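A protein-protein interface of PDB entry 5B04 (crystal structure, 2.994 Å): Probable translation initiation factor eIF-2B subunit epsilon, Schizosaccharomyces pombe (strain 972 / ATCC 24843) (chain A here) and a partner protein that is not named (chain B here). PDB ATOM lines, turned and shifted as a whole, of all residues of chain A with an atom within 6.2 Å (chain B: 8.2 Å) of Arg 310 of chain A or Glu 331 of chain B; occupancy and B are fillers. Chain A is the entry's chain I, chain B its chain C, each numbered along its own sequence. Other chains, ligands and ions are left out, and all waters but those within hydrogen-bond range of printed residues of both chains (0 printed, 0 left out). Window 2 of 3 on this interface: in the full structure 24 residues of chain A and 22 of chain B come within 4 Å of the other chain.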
ATOM      1  N   TYR A 308      17.194  23.898  -7.621  1.00  0.00           N
ATOM      2  CA  TYR A 308      17.618  23.376  -8.914  1.00  0.00           C
ATOM      3  C   TYR A 308      18.776  24.194  -9.465  1.00  0.00           C
ATOM      4  O   TYR A 308      18.792  25.421  -9.365  1.00  0.00           O
ATOM      5  CB  TYR A 308      16.463  23.368  -9.921  1.00  0.00           C
ATOM      6  CG  TYR A 308      16.862  22.847 -11.290  1.00  0.00           C
ATOM      7  CD1 TYR A 308      17.346  23.705 -12.272  1.00  0.00           C
ATOM      8  CD2 TYR A 308      16.766  21.496 -11.594  1.00  0.00           C
ATOM      9  CE1 TYR A 308      17.719  23.232 -13.516  1.00  0.00           C
ATOM     10  CE2 TYR A 308      17.134  21.013 -12.838  1.00  0.00           C
ATOM     11  CZ  TYR A 308      17.609  21.886 -13.794  1.00  0.00           C
ATOM     12  OH  TYR A 308      17.977  21.411 -15.034  1.00  0.00           O
ATOM     13  N   GLN A 309      19.745  23.500 -10.050  1.00  0.00           N
ATOM     14  CA  GLN A 309      20.852  24.146 -10.738  1.00  0.00           C
ATOM     15  C   GLN A 309      21.091  23.442 -12.066  1.00  0.00           C
ATOM     16  O   GLN A 309      20.592  22.337 -12.284  1.00  0.00           O
ATOM     17  CB  GLN A 309      22.111  24.134  -9.871  1.00  0.00           C
ATOM     18  CG  GLN A 309      22.029  25.066  -8.671  1.00  0.00           C
ATOM     19  CD  GLN A 309      22.962  24.664  -7.549  1.00  0.00           C
ATOM     20  OE1 GLN A 309      22.524  24.173  -6.509  1.00  0.00           O
ATOM     21  NE2 GLN A 309      24.258  24.875  -7.752  1.00  0.00           N
ATOM     22  N   ARG A 310      21.844  24.087 -12.950  1.00  0.00           N
ATOM     23  CA  ARG A 310      22.057  23.575 -14.300  1.00  0.00           C
ATOM     24  C   ARG A 310      22.662  22.175 -14.299  1.00  0.00           C
ATOM     25  O   ARG A 310      23.386  21.803 -13.374  1.00  0.00           O
ATOM     26  CB  ARG A 310      22.941  24.536 -15.095  1.00  0.00           C
ATOM     27  CG  ARG A 310      22.302  25.897 -15.303  1.00  0.00           C
ATOM     28  CD  ARG A 310      23.178  26.812 -16.135  1.00  0.00           C
ATOM     29  NE  ARG A 310      22.471  28.035 -16.504  1.00  0.00           N
ATOM     30  CZ  ARG A 310      21.720  28.161 -17.594  1.00  0.00           C
ATOM     31  NH1 ARG A 310      21.580  27.139 -18.426  1.00  0.00           N
ATOM     32  NH2 ARG A 310      21.111  29.310 -17.852  1.00  0.00           N
ATOM     33  N   HIS A 311      22.339  21.412 -15.341  1.00  0.00           N
ATOM     34  CA  HIS A 311      22.737  20.012 -15.474  1.00  0.00           C
ATOM     35  C   HIS A 311      22.139  19.162 -14.355  1.00  0.00           C
ATOM     36  O   HIS A 311      22.738  18.178 -13.918  1.00  0.00           O
ATOM     37  CB  HIS A 311      24.259  19.879 -15.502  1.00  0.00           C
ATOM     38  CG  HIS A 311      24.925  20.840 -16.435  1.00  0.00           C
ATOM     39  ND1 HIS A 311      25.508  22.011 -16.005  1.00  0.00           N
ATOM     40  CD2 HIS A 311      25.082  20.812 -17.780  1.00  0.00           C
ATOM     41  CE1 HIS A 311      26.006  22.660 -17.044  1.00  0.00           C
ATOM     42  NE2 HIS A 311      25.759  21.954 -18.132  1.00  0.00           N
ATOM     43  N   GLN A 312      20.950  19.560 -13.907  1.00  0.00           N
ATOM     44  CA  GLN A 312      20.165  18.804 -12.933  1.00  0.00           C
ATOM     45  C   GLN A 312      20.919  18.523 -11.635  1.00  0.00           C
ATOM     46  O   GLN A 312      21.013  17.377 -11.199  1.00  0.00           O
ATOM     47  CB  GLN A 312      19.688  17.488 -13.554  1.00  0.00           C
ATOM     48  CG  GLN A 312      18.777  17.672 -14.758  1.00  0.00           C
ATOM     49  CD  GLN A 312      19.313  16.997 -16.003  1.00  0.00           C
ATOM     50  OE1 GLN A 312      20.525  16.871 -16.180  1.00  0.00           O
ATOM     51  NE2 GLN A 312      18.412  16.559 -16.874  1.00  0.00           N
ATOM     52  N   ILE A 313      21.448  19.575 -11.021  1.00  0.00           N
ATOM     53  CA  ILE A 313      22.112  19.448  -9.729  1.00  0.00           C
ATOM     54  C   ILE A 313      21.247  20.054  -8.629  1.00  0.00           C
ATOM     55  O   ILE A 313      20.943  21.246  -8.650  1.00  0.00           O
ATOM     56  CB  ILE A 313      23.496  20.120  -9.731  1.00  0.00           C
ATOM     57  CG1 ILE A 313      24.453  19.351 -10.643  1.00  0.00           C
ATOM     58  CG2 ILE A 313      24.054  20.195  -8.319  1.00  0.00           C
ATOM     59  CD1 ILE A 313      25.839  19.949 -10.721  1.00  0.00           C
ATOM     60  N   ALA A 329      27.002  16.252 -13.259  1.00  0.00           N
ATOM     61  CA  ALA A 329      25.577  16.342 -13.562  1.00  0.00           C
ATOM     62  C   ALA A 329      24.735  15.280 -12.857  1.00  0.00           C
ATOM     63  O   ALA A 329      25.243  14.234 -12.452  1.00  0.00           O
ATOM     64  CB  ALA A 329      25.363  16.259 -15.065  1.00  0.00           C
ATOM     65  N   THR B  77       8.441  31.790  -6.351  1.00  0.00           N
ATOM     66  CA  THR B  77       8.438  32.532  -7.609  1.00  0.00           C
ATOM     67  C   THR B  77       7.052  33.055  -7.973  1.00  0.00           C
ATOM     68  O   THR B  77       6.856  33.613  -9.052  1.00  0.00           O
ATOM     69  CB  THR B  77       8.972  31.676  -8.769  1.00  0.00           C
ATOM     70  OG1 THR B  77       8.287  30.418  -8.797  1.00  0.00           O
ATOM     71  CG2 THR B  77      10.463  31.433  -8.601  1.00  0.00           C
ATOM     72  N   PRO B 327      16.661  40.576  -8.085  1.00  0.00           N
ATOM     73  CA  PRO B 327      17.139  39.415  -8.844  1.00  0.00           C
ATOM     74  C   PRO B 327      18.641  39.192  -8.701  1.00  0.00           C
ATOM     75  O   PRO B 327      19.382  39.410  -9.660  1.00  0.00           O
ATOM     76  CB  PRO B 327      16.782  39.771 -10.290  1.00  0.00           C
ATOM     77  CG  PRO B 327      16.733  41.258 -10.309  1.00  0.00           C
ATOM     78  CD  PRO B 327      16.193  41.657  -8.969  1.00  0.00           C
ATOM     79  N   TYR B 328      19.080  38.766  -7.521  1.00  0.00           N
ATOM     80  CA  TYR B 328      20.492  38.487  -7.285  1.00  0.00           C
ATOM     81  C   TYR B 328      20.995  37.373  -8.194  1.00  0.00           C
ATOM     82  O   TYR B 328      22.035  37.505  -8.839  1.00  0.00           O
ATOM     83  CB  TYR B 328      20.733  38.112  -5.822  1.00  0.00           C
ATOM     84  CG  TYR B 328      20.724  39.284  -4.868  1.00  0.00           C
ATOM     85  CD1 TYR B 328      21.771  40.197  -4.851  1.00  0.00           C
ATOM     86  CD2 TYR B 328      19.677  39.471  -3.974  1.00  0.00           C
ATOM     87  CE1 TYR B 328      21.771  41.267  -3.977  1.00  0.00           C
ATOM     88  CE2 TYR B 328      19.669  40.537  -3.097  1.00  0.00           C
ATOM     89  CZ  TYR B 328      20.718  41.432  -3.102  1.00  0.00           C
ATOM     90  OH  TYR B 328      20.714  42.497  -2.229  1.00  0.00           O
ATOM     91  N   ASP B 329      20.249  36.275  -8.240  1.00  0.00           N
ATOM     92  CA  ASP B 329      20.606  35.143  -9.086  1.00  0.00           C
ATOM     93  C   ASP B 329      19.410  34.701  -9.919  1.00  0.00           C
ATOM     94  O   ASP B 329      18.412  34.221  -9.382  1.00  0.00           O
ATOM     95  CB  ASP B 329      21.119  33.979  -8.237  1.00  0.00           C
ATOM     96  CG  ASP B 329      21.888  32.954  -9.051  1.00  0.00           C
ATOM     97  OD1 ASP B 329      21.810  32.994 -10.297  1.00  0.00           O
ATOM     98  OD2 ASP B 329      22.570  32.102  -8.445  1.00  0.00           O
ATOM     99  N   LEU B 330      19.521  34.862 -11.234  1.00  0.00           N
ATOM    100  CA  LEU B 330      18.451  34.476 -12.148  1.00  0.00           C
ATOM    101  C   LEU B 330      18.241  32.964 -12.160  1.00  0.00           C
ATOM    102  O   LEU B 330      17.174  32.482 -12.535  1.00  0.00           O
ATOM    103  CB  LEU B 330      18.754  34.974 -13.563  1.00  0.00           C
ATOM    104  CG  LEU B 330      18.715  36.488 -13.777  1.00  0.00           C
ATOM    105  CD1 LEU B 330      19.106  36.836 -15.204  1.00  0.00           C
ATOM    106  CD2 LEU B 330      17.338  37.042 -13.447  1.00  0.00           C
ATOM    107  N   GLU B 331      19.264  32.223 -11.742  1.00  0.00           N
ATOM    108  CA  GLU B 331      19.199  30.765 -11.701  1.00  0.00           C
ATOM    109  C   GLU B 331      18.130  30.261 -10.733  1.00  0.00           C
ATOM    110  O   GLU B 331      17.635  29.143 -10.870  1.00  0.00           O
ATOM    111  CB  GLU B 331      20.562  30.183 -11.317  1.00  0.00           C
ATOM    112  CG  GLU B 331      21.599  30.241 -12.426  1.00  0.00           C
ATOM    113  CD  GLU B 331      21.373  29.183 -13.489  1.00  0.00           C
ATOM    114  OE1 GLU B 331      21.117  28.017 -13.121  1.00  0.00           O
ATOM    115  OE2 GLU B 331      21.448  29.517 -14.691  1.00  0.00           O
ATOM    116  N   SER B 332      17.780  31.092  -9.756  1.00  0.00           N
ATOM    117  CA  SER B 332      16.768  30.735  -8.768  1.00  0.00           C
ATOM    118  C   SER B 332      15.388  31.239  -9.179  1.00  0.00           C
ATOM    119  O   SER B 332      14.370  30.792  -8.654  1.00  0.00           O
ATOM    120  CB  SER B 332      17.141  31.300  -7.396  1.00  0.00           C
ATOM    121  OG  SER B 332      17.228  32.714  -7.435  1.00  0.00           O
ATOM    122  N   ILE B 333      15.367  32.169 -10.127  1.00  0.00           N
ATOM    123  CA  ILE B 333      14.129  32.795 -10.570  1.00  0.00           C
ATOM    124  C   ILE B 333      13.457  31.996 -11.683  1.00  0.00           C
ATOM    125  O   ILE B 333      12.246  31.774 -11.657  1.00  0.00           O
ATOM    126  CB  ILE B 333      14.387  34.236 -11.044  1.00  0.00           C
ATOM    127  CG1 ILE B 333      14.636  35.140  -9.836  1.00  0.00           C
ATOM    128  CG2 ILE B 333      13.218  34.757 -11.859  1.00  0.00           C
ATOM    129  CD1 ILE B 333      15.256  36.466 -10.186  1.00  0.00           C
ATOM    130  N   ILE B 334      14.246  31.559 -12.659  1.00  0.00           N
ATOM    131  CA  ILE B 334      13.721  30.748 -13.751  1.00  0.00           C
ATOM    132  C   ILE B 334      13.351  29.354 -13.251  1.00  0.00           C
ATOM    133  O   ILE B 334      14.178  28.649 -12.673  1.00  0.00           O
ATOM    134  CB  ILE B 334      14.729  30.624 -14.917  1.00  0.00           C
ATOM    135  CG1 ILE B 334      14.723  31.890 -15.778  1.00  0.00           C
ATOM    136  CG2 ILE B 334      14.394  29.425 -15.791  1.00  0.00           C
ATOM    137  CD1 ILE B 334      15.498  33.052 -15.197  1.00  0.00           C
ATOM    138  N   GLN B 335      12.097  28.970 -13.464  1.00  0.00           N
ATOM    139  CA  GLN B 335      11.637  27.636 -13.106  1.00  0.00           C
ATOM    140  C   GLN B 335      11.636  26.733 -14.331  1.00  0.00           C
ATOM    141  O   GLN B 335      11.463  27.201 -15.456  1.00  0.00           O
ATOM    142  CB  GLN B 335      10.240  27.692 -12.487  1.00  0.00           C
ATOM    143  CG  GLN B 335      10.167  28.472 -11.188  1.00  0.00           C
ATOM    144  CD  GLN B 335      11.116  27.935 -10.137  1.00  0.00           C
ATOM    145  OE1 GLN B 335      11.890  28.685  -9.543  1.00  0.00           O
ATOM    146  NE2 GLN B 335      11.058  26.630  -9.899  1.00  0.00           N
ATOM    147  N   LEU B 336      11.834  25.439 -14.111  1.00  0.00           N
ATOM    148  CA  LEU B 336      11.822  24.472 -15.200  1.00  0.00           C
ATOM    149  C   LEU B 336      10.693  23.468 -15.020  1.00  0.00           C
ATOM    150  O   LEU B 336      10.590  22.816 -13.982  1.00  0.00           O
ATOM    151  CB  LEU B 336      13.164  23.740 -15.299  1.00  0.00           C
ATOM    152  CG  LEU B 336      14.320  24.427 -16.033  1.00  0.00           C
ATOM    153  CD1 LEU B 336      14.843  25.633 -15.266  1.00  0.00           C
ATOM    154  CD2 LEU B 336      15.442  23.437 -16.309  1.00  0.00           C
ATOM    155  N   GLU B 355      20.080  15.780 -22.621  1.00  0.00           N
ATOM    156  CA  GLU B 355      19.537  16.629 -21.573  1.00  0.00           C
ATOM    157  C   GLU B 355      18.431  17.507 -22.147  1.00  0.00           C
ATOM    158  O   GLU B 355      18.686  18.351 -23.005  1.00  0.00           O
ATOM    159  CB  GLU B 355      20.643  17.488 -20.958  1.00  0.00           C
ATOM    160  CG  GLU B 355      20.178  18.465 -19.895  1.00  0.00           C
ATOM    161  CD  GLU B 355      21.338  19.170 -19.216  1.00  0.00           C
ATOM    162  OE1 GLU B 355      21.868  18.623 -18.227  1.00  0.00           O
ATOM    163  OE2 GLU B 355      21.723  20.266 -19.674  1.00  0.00           O
ATOM    164  N   LEU B 357      15.583  20.356 -21.522  1.00  0.00           N
ATOM    165  CA  LEU B 357      15.295  21.433 -20.584  1.00  0.00           C
ATOM    166  C   LEU B 357      14.117  22.292 -21.032  1.00  0.00           C
ATOM    167  O   LEU B 357      14.130  22.859 -22.123  1.00  0.00           O
ATOM    168  CB  LEU B 357      16.533  22.309 -20.399  1.00  0.00           C
ATOM    169  CG  LEU B 357      17.810  21.565 -20.004  1.00  0.00           C
ATOM    170  CD1 LEU B 357      19.006  22.503 -20.012  1.00  0.00           C
ATOM    171  CD2 LEU B 357      17.643  20.913 -18.641  1.00  0.00           C
ATOM    172  N   PRO B 359      12.325  25.416 -19.505  1.00  0.00           N
ATOM    173  CA  PRO B 359      12.004  26.533 -18.612  1.00  0.00           C
ATOM    174  C   PRO B 359      10.728  27.229 -19.067  1.00  0.00           C
ATOM    175  O   PRO B 359      10.531  27.391 -20.272  1.00  0.00           O
ATOM    176  CB  PRO B 359      13.219  27.451 -18.751  1.00  0.00           C
ATOM    177  CG  PRO B 359      13.722  27.185 -20.129  1.00  0.00           C
ATOM    178  CD  PRO B 359      13.448  25.729 -20.407  1.00  0.00           C
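Hydrophobic or aromatic side chains of chain B within 4 Å of the printed part of chain A: Leu 336 and Leu 357. Printed residues of chain A that touch a printed residue of chain B: Tyr 308, Arg 310, His 311 and Gln 312. Hydrophobic or aromatic side chains of chain A that line the printed part of chain B: Tyr 308 and His 311. Among the printed residues, 5 pairs touch across the chains.
The guanidinium group of Arg 310 of chain A lies within salt-bridge range of the side-chain carboxylate of Glu 331 of chain B, 2.6 Å away. The side-chain amide oxygen of Gln 312 of chain A sits close to the side-chain carboxylate of Glu 355 of chain B.
Of the printed residues of chain A, Glu 331 of chain B touches Arg 310. Printed residues of chain B within 4 Å of His 311 of chain A: Glu 355. Of the printed residues of chain B, Gln 312 of chain A touches Glu 355 (3.0 Å). Of the printed residues of chain A, Leu 357 of chain B touches Tyr 308 (3.7 Å). The nearest residue of chain A that does not touch Glu 331 of chain B is Tyr 308 of chain A (4.2 Å). The nearest printed residue of chain A that does not touch Glu 355 of chain B is Ala 329 of chain A (5.3 Å).
Among the printed residues, merely in contact across the chains: His 311 of chain A with Glu 355 of chain B (3.2 Å), Tyr 308 of chain A with Leu 336 of chain B (3.5 Å) and Tyr 308 of chain A with Leu 357 of chain B (3.7 Å).
The backbone NH (N) of Glu 331 of chain B is in hydrogen-bond range of the side-chain carboxylate (OD1) of Asp 329 of chain B (3.0 Å).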
